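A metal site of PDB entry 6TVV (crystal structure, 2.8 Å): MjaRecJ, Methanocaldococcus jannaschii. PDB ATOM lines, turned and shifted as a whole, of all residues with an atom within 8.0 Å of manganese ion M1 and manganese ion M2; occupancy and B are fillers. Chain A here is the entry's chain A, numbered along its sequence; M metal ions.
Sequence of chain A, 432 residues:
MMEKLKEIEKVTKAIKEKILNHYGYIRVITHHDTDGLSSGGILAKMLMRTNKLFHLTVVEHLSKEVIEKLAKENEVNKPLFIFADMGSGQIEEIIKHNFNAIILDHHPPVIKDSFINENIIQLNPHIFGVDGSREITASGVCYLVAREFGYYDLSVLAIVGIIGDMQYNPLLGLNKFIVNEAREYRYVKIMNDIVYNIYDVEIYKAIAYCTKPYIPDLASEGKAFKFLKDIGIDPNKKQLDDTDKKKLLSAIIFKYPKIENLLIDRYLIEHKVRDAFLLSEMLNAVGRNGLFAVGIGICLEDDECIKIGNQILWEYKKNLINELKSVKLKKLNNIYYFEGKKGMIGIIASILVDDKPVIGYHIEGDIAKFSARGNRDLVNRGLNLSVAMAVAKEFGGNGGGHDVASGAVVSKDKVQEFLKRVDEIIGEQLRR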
ATOM      1  N   HIS A  31     -18.383  21.864   6.042  1.00  0.00           N
ATOM      2  CA  HIS A  31     -19.419  21.084   5.328  1.00  0.00           C
ATOM      3  C   HIS A  31     -19.736  21.840   4.027  1.00  0.00           C
ATOM      4  O   HIS A  31     -19.361  23.037   3.921  1.00  0.00           O
ATOM      5  CB  HIS A  31     -20.555  20.900   6.336  1.00  0.00           C
ATOM      6  CG  HIS A  31     -21.443  19.729   6.122  1.00  0.00           C
ATOM      7  ND1 HIS A  31     -22.818  19.858   6.111  1.00  0.00           N
ATOM      8  CD2 HIS A  31     -21.168  18.424   5.957  1.00  0.00           C
ATOM      9  CE1 HIS A  31     -23.357  18.683   5.919  1.00  0.00           C
ATOM     10  NE2 HIS A  31     -22.358  17.787   5.793  1.00  0.00           N
ATOM     11  N   HIS A  32     -20.361  21.165   3.076  1.00  0.00           N
ATOM     12  CA  HIS A  32     -20.563  21.662   1.684  1.00  0.00           C
ATOM     13  C   HIS A  32     -21.885  22.421   1.547  1.00  0.00           C
ATOM     14  O   HIS A  32     -22.104  22.965   0.472  1.00  0.00           O
ATOM     15  CB  HIS A  32     -20.505  20.503   0.698  1.00  0.00           C
ATOM     16  CG  HIS A  32     -21.632  19.530   0.844  1.00  0.00           C
ATOM     17  ND1 HIS A  32     -22.037  19.028   2.072  1.00  0.00           N
ATOM     18  CD2 HIS A  32     -22.454  18.995  -0.076  1.00  0.00           C
ATOM     19  CE1 HIS A  32     -23.066  18.228   1.912  1.00  0.00           C
ATOM     20  NE2 HIS A  32     -23.330  18.184   0.595  1.00  0.00           N
ATOM     21  N   ASP A  33     -22.731  22.414   2.594  1.00  0.00           N
ATOM     22  CA  ASP A  33     -24.042  23.124   2.702  1.00  0.00           C
ATOM     23  C   ASP A  33     -23.762  24.635   2.926  1.00  0.00           C
ATOM     24  O   ASP A  33     -22.654  24.992   3.308  1.00  0.00           O
ATOM     25  CB  ASP A  33     -24.934  22.444   3.775  1.00  0.00           C
ATOM     26  CG  ASP A  33     -24.399  22.404   5.220  1.00  0.00           C
ATOM     27  OD1 ASP A  33     -23.301  22.950   5.472  1.00  0.00           O
ATOM     28  OD2 ASP A  33     -25.059  21.839   6.112  1.00  0.00           O
ATOM     29  N   THR A  34     -24.761  25.492   2.724  1.00  0.00           N
ATOM     30  CA  THR A  34     -24.690  26.945   3.027  1.00  0.00           C
ATOM     31  C   THR A  34     -24.163  27.186   4.433  1.00  0.00           C
ATOM     32  O   THR A  34     -23.376  28.129   4.598  1.00  0.00           O
ATOM     33  CB  THR A  34     -26.035  27.640   2.807  1.00  0.00           C
ATOM     34  OG1 THR A  34     -26.410  27.379   1.457  1.00  0.00           O
ATOM     35  CG2 THR A  34     -26.000  29.123   3.042  1.00  0.00           C
ATOM     36  N   ASP A  35     -24.571  26.398   5.422  1.00  0.00           N
ATOM     37  CA  ASP A  35     -24.118  26.607   6.837  1.00  0.00           C
ATOM     38  C   ASP A  35     -22.611  26.311   6.928  1.00  0.00           C
ATOM     39  O   ASP A  35     -21.907  27.004   7.692  1.00  0.00           O
ATOM     40  CB  ASP A  35     -24.956  25.773   7.803  1.00  0.00           C
ATOM     41  CG  ASP A  35     -24.741  26.058   9.282  1.00  0.00           C
ATOM     42  OD1 ASP A  35     -24.525  27.273   9.581  1.00  0.00           O
ATOM     43  OD2 ASP A  35     -24.864  25.053  10.130  1.00  0.00           O
ATOM     44  N   GLY A  36     -22.125  25.373   6.115  1.00  0.00           N
ATOM     45  CA  GLY A  36     -20.712  24.953   6.106  1.00  0.00           C
ATOM     46  C   GLY A  36     -19.838  25.971   5.419  1.00  0.00           C
ATOM     47  O   GLY A  36     -18.806  26.388   5.992  1.00  0.00           O
ATOM     48  N   SER A  39     -19.683  29.174   7.359  1.00  0.00           N
ATOM     49  CA  SER A  39     -18.794  28.870   8.501  1.00  0.00           C
ATOM     50  C   SER A  39     -17.355  29.007   8.013  1.00  0.00           C
ATOM     51  O   SER A  39     -16.618  29.759   8.643  1.00  0.00           O
ATOM     52  CB  SER A  39     -19.073  27.506   9.064  1.00  0.00           C
ATOM     53  OG  SER A  39     -20.293  27.517   9.792  1.00  0.00           O
ATOM     54  N   GLU A  60     -18.022  16.028   2.772  1.00  0.00           N
ATOM     55  CA  GLU A  60     -19.460  15.684   2.612  1.00  0.00           C
ATOM     56  C   GLU A  60     -19.944  15.140   3.963  1.00  0.00           C
ATOM     57  O   GLU A  60     -20.850  15.738   4.541  1.00  0.00           O
ATOM     58  CB  GLU A  60     -19.677  14.683   1.476  1.00  0.00           C
ATOM     59  CG  GLU A  60     -18.930  15.040   0.201  1.00  0.00           C
ATOM     60  CD  GLU A  60     -19.808  15.626  -0.888  1.00  0.00           C
ATOM     61  OE1 GLU A  60     -20.439  14.841  -1.618  1.00  0.00           O
ATOM     62  OE2 GLU A  60     -19.850  16.868  -0.994  1.00  0.00           O
ATOM     63  N   ALA A  84     -16.168  22.658  11.804  1.00  0.00           N
ATOM     64  CA  ALA A  84     -17.322  23.565  11.676  1.00  0.00           C
ATOM     65  C   ALA A  84     -18.576  22.739  11.870  1.00  0.00           C
ATOM     66  O   ALA A  84     -18.786  22.258  12.996  1.00  0.00           O
ATOM     67  CB  ALA A  84     -17.301  24.258  10.355  1.00  0.00           C
ATOM     68  N   ASP A  85     -19.395  22.550  10.856  1.00  0.00           N
ATOM     69  CA  ASP A  85     -20.819  22.151  11.083  1.00  0.00           C
ATOM     70  C   ASP A  85     -20.815  20.615  11.279  1.00  0.00           C
ATOM     71  O   ASP A  85     -21.472  19.889  10.512  1.00  0.00           O
ATOM     72  CB  ASP A  85     -21.635  22.855   9.992  1.00  0.00           C
ATOM     73  CG  ASP A  85     -22.966  22.288   9.556  1.00  0.00           C
ATOM     74  OD1 ASP A  85     -23.850  22.119  10.448  1.00  0.00           O
ATOM     75  OD2 ASP A  85     -23.128  22.110   8.307  1.00  0.00           O
ATOM     76  N   MET A  86     -20.059  20.139  12.278  1.00  0.00           N
ATOM     77  CA  MET A  86     -19.654  18.712  12.453  1.00  0.00           C
ATOM     78  C   MET A  86     -18.665  18.589  13.619  1.00  0.00           C
ATOM     79  O   MET A  86     -18.145  19.603  14.027  1.00  0.00           O
ATOM     80  CB  MET A  86     -18.967  18.128  11.225  1.00  0.00           C
ATOM     81  CG  MET A  86     -17.550  18.648  11.029  1.00  0.00           C
ATOM     82  SD  MET A  86     -16.852  18.330   9.382  1.00  0.00           S
ATOM     83  CE  MET A  86     -18.234  18.693   8.304  1.00  0.00           C
ATOM     84  N   ASP A 105     -20.201  23.255  16.563  1.00  0.00           N
ATOM     85  CA  ASP A 105     -21.288  22.392  16.035  1.00  0.00           C
ATOM     86  C   ASP A 105     -22.593  22.812  16.723  1.00  0.00           C
ATOM     87  O   ASP A 105     -22.551  23.646  17.661  1.00  0.00           O
ATOM     88  CB  ASP A 105     -20.929  20.908  16.208  1.00  0.00           C
ATOM     89  CG  ASP A 105     -21.602  19.959  15.236  1.00  0.00           C
ATOM     90  OD1 ASP A 105     -22.498  20.438  14.512  1.00  0.00           O
ATOM     91  OD2 ASP A 105     -21.238  18.731  15.237  1.00  0.00           O
ATOM     92  N   HIS A 106     -23.702  22.324  16.202  1.00  0.00           N
ATOM     93  CA  HIS A 106     -25.084  22.573  16.709  1.00  0.00           C
ATOM     94  C   HIS A 106     -25.925  21.307  16.516  1.00  0.00           C
ATOM     95  O   HIS A 106     -27.091  21.333  16.939  1.00  0.00           O
ATOM     96  CB  HIS A 106     -25.708  23.790  16.006  1.00  0.00           C
ATOM     97  CG  HIS A 106     -26.042  23.577  14.566  1.00  0.00           C
ATOM     98  ND1 HIS A 106     -27.306  23.753  14.090  1.00  0.00           N
ATOM     99  CD2 HIS A 106     -25.284  23.239  13.496  1.00  0.00           C
ATOM    100  CE1 HIS A 106     -27.327  23.520  12.787  1.00  0.00           C
ATOM    101  NE2 HIS A 106     -26.111  23.208  12.384  1.00  0.00           N
ATOM    102  N   HIS A 107     -25.355  20.274  15.905  1.00  0.00           N
ATOM    103  CA  HIS A 107     -25.915  18.897  15.868  1.00  0.00           C
ATOM    104  C   HIS A 107     -25.984  18.384  17.314  1.00  0.00           C
ATOM    105  O   HIS A 107     -25.291  18.865  18.188  1.00  0.00           O
ATOM    106  CB  HIS A 107     -25.090  18.011  14.911  1.00  0.00           C
ATOM    107  CG  HIS A 107     -25.164  18.408  13.466  1.00  0.00           C
ATOM    108  ND1 HIS A 107     -25.445  17.497  12.463  1.00  0.00           N
ATOM    109  CD2 HIS A 107     -24.941  19.595  12.850  1.00  0.00           C
ATOM    110  CE1 HIS A 107     -25.415  18.108  11.304  1.00  0.00           C
ATOM    111  NE2 HIS A 107     -25.107  19.408  11.508  1.00  0.00           N
ATOM    112  N   GLY A 132     -29.977  23.424  18.198  1.00  0.00           N
ATOM    113  CA  GLY A 132     -29.404  23.598  16.845  1.00  0.00           C
ATOM    114  C   GLY A 132     -30.391  23.169  15.802  1.00  0.00           C
ATOM    115  O   GLY A 132     -29.969  22.926  14.658  1.00  0.00           O
ATOM    116  N   ILE A 136     -29.995  28.273  16.550  1.00  0.00           N
ATOM    117  CA  ILE A 136     -28.535  28.488  16.261  1.00  0.00           C
ATOM    118  C   ILE A 136     -28.100  27.520  15.148  1.00  0.00           C
ATOM    119  O   ILE A 136     -28.640  26.413  15.074  1.00  0.00           O
ATOM    120  CB  ILE A 136     -27.696  28.332  17.546  1.00  0.00           C
ATOM    121  CG1 ILE A 136     -26.257  28.830  17.422  1.00  0.00           C
ATOM    122  CG2 ILE A 136     -27.688  26.875  17.998  1.00  0.00           C
ATOM    123  CD1 ILE A 136     -26.123  30.317  17.445  1.00  0.00           C
ATOM    124  N   THR A 137     -27.128  27.949  14.341  1.00  0.00           N
ATOM    125  CA  THR A 137     -26.480  27.226  13.228  1.00  0.00           C
ATOM    126  C   THR A 137     -24.968  27.286  13.453  1.00  0.00           C
ATOM    127  O   THR A 137     -24.533  27.995  14.386  1.00  0.00           O
ATOM    128  CB  THR A 137     -26.851  27.858  11.875  1.00  0.00           C
ATOM    129  OG1 THR A 137     -26.627  29.268  11.934  1.00  0.00           O
ATOM    130  CG2 THR A 137     -28.310  27.667  11.504  1.00  0.00           C
ATOM    131  N   ALA A 138     -24.187  26.604  12.624  1.00  0.00           N
ATOM    132  CA  ALA A 138     -22.714  26.594  12.742  1.00  0.00           C
ATOM    133  C   ALA A 138     -22.151  27.995  12.472  1.00  0.00           C
ATOM    134  O   ALA A 138     -21.301  28.488  13.249  1.00  0.00           O
ATOM    135  CB  ALA A 138     -22.144  25.576  11.804  1.00  0.00           C
ATOM    136  N   SER A 139     -22.619  28.609  11.391  1.00  0.00           N
ATOM    137  CA  SER A 139     -22.316  30.014  11.023  1.00  0.00           C
ATOM    138  C   SER A 139     -22.471  30.894  12.253  1.00  0.00           C
ATOM    139  O   SER A 139     -21.570  31.694  12.545  1.00  0.00           O
ATOM    140  CB  SER A 139     -23.215  30.461   9.934  1.00  0.00           C
ATOM    141  OG  SER A 139     -24.546  30.208  10.324  1.00  0.00           O
ATOM    142  N   GLY A 161     -26.120  31.542   7.005  1.00  0.00           N
ATOM    143  CA  GLY A 161     -26.241  30.176   7.563  1.00  0.00           C
ATOM    144  C   GLY A 161     -27.602  29.949   8.173  1.00  0.00           C
ATOM    145  O   GLY A 161     -28.205  28.855   7.959  1.00  0.00           O
ATOM    146  N   GLY A 164     -29.684  29.391   5.351  1.00  0.00           N
ATOM    147  CA  GLY A 164     -29.248  28.100   4.793  1.00  0.00           C
ATOM    148  C   GLY A 164     -29.953  26.947   5.472  1.00  0.00           C
ATOM    149  O   GLY A 164     -30.528  26.125   4.761  1.00  0.00           O
ATOM    150  N   ASP A 165     -29.916  26.902   6.811  1.00  0.00           N
ATOM    151  CA  ASP A 165     -30.410  25.769   7.643  1.00  0.00           C
ATOM    152  C   ASP A 165     -31.900  25.965   7.958  1.00  0.00           C
ATOM    153  O   ASP A 165     -32.407  25.211   8.793  1.00  0.00           O
ATOM    154  CB  ASP A 165     -29.591  25.635   8.931  1.00  0.00           C
ATOM    155  CG  ASP A 165     -28.336  24.787   8.817  1.00  0.00           C
ATOM    156  OD1 ASP A 165     -28.122  24.201   7.735  1.00  0.00           O
ATOM    157  OD2 ASP A 165     -27.572  24.721   9.818  1.00  0.00           O
ATOM    158  N   GLN A 167     -33.745  28.431   9.557  1.00  0.00           N
ATOM    159  CA  GLN A 167     -34.039  28.821  10.972  1.00  0.00           C
ATOM    160  C   GLN A 167     -34.450  30.299  11.051  1.00  0.00           C
ATOM    161  O   GLN A 167     -34.252  30.907  12.136  1.00  0.00           O
ATOM    162  CB  GLN A 167     -32.834  28.528  11.878  1.00  0.00           C
ATOM    163  CG  GLN A 167     -32.446  27.057  11.878  1.00  0.00           C
ATOM    164  CD  GLN A 167     -31.504  26.667  13.000  1.00  0.00           C
ATOM    165  OE1 GLN A 167     -31.129  27.496  13.840  1.00  0.00           O
ATOM    166  NE2 GLN A 167     -31.095  25.404  12.985  1.00  0.00           N
HETATM  167 MN    MN M   1     -25.994  22.888   9.790  1.00  0.00          MN
HETATM  168 MN    MN M   2     -24.940  20.645   7.697  1.00  0.00          MN
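His 107 touches manganese ion M1 (NE2 to MN, 3.98 Å).
Along chain A the residues within 4 Å of manganese ion M1 span positions 33 to 165.
The nearest printed residue that does not touch manganese ion M1 is Ala 138 (5.0 Å).
A ring nitrogen (NE2) of His 31 sits at hydrogen-bond distance from the backbone carbonyl oxygen (O) of Glu 60 (2.8 Å).
The side-chain carboxylate (OD1) of Asp 35 is in hydrogen-bond range of the backbone NH (N) of Ala 138 (3.1 Å).
The backbone NH of Gly 36 is in hydrogen-bond range of the side-chain carboxylate of Asp 33.
O of Ile 136 lies within hydrogen-bond range of ND1 of His 106.
A ring nitrogen (ND1) of His 31 sits close to the side-chain carboxylate of Asp 33, 3.2 Å away.
N of His 107 lies close to OD1 of Asp 105, at 3.2 Å.
The side-chain carboxylate (OD1) of Asp 35 lies within hydrogen-bond range of the backbone NH (N) of Ser 139 (2.9 Å).
The side-chain hydroxyl (OG) of Ser 39 sits at hydrogen-bond distance from the backbone carbonyl oxygen (O) of Asp 35, 2.7 Å away.
Within 4 Å of manganese ion M2: His 31, Asp 33 and Asp 85.
The nearest printed residue that does not touch manganese ion M2 is His 107 (4.01 Å).
Manganese ion M1 is bound by the side-chain carboxylate (OD1) of Asp 85, at 2.4 Å.
OD2 of Asp 165 is bound to manganese ion M1, 2.4 Å away.
OD2 of Asp 35 is bound to manganese ion M1, 2.5 Å away.
A ring nitrogen (NE2) of His 106 binds manganese ion M1 (2.6 Å).
Manganese ion M2 is bound by OD2 of Asp 33 (2.0 Å) and OD2 of Asp 85 (2.4 Å).
Slightly farther from manganese ion M2 lies ND1 of His 31 (2.8 Å).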
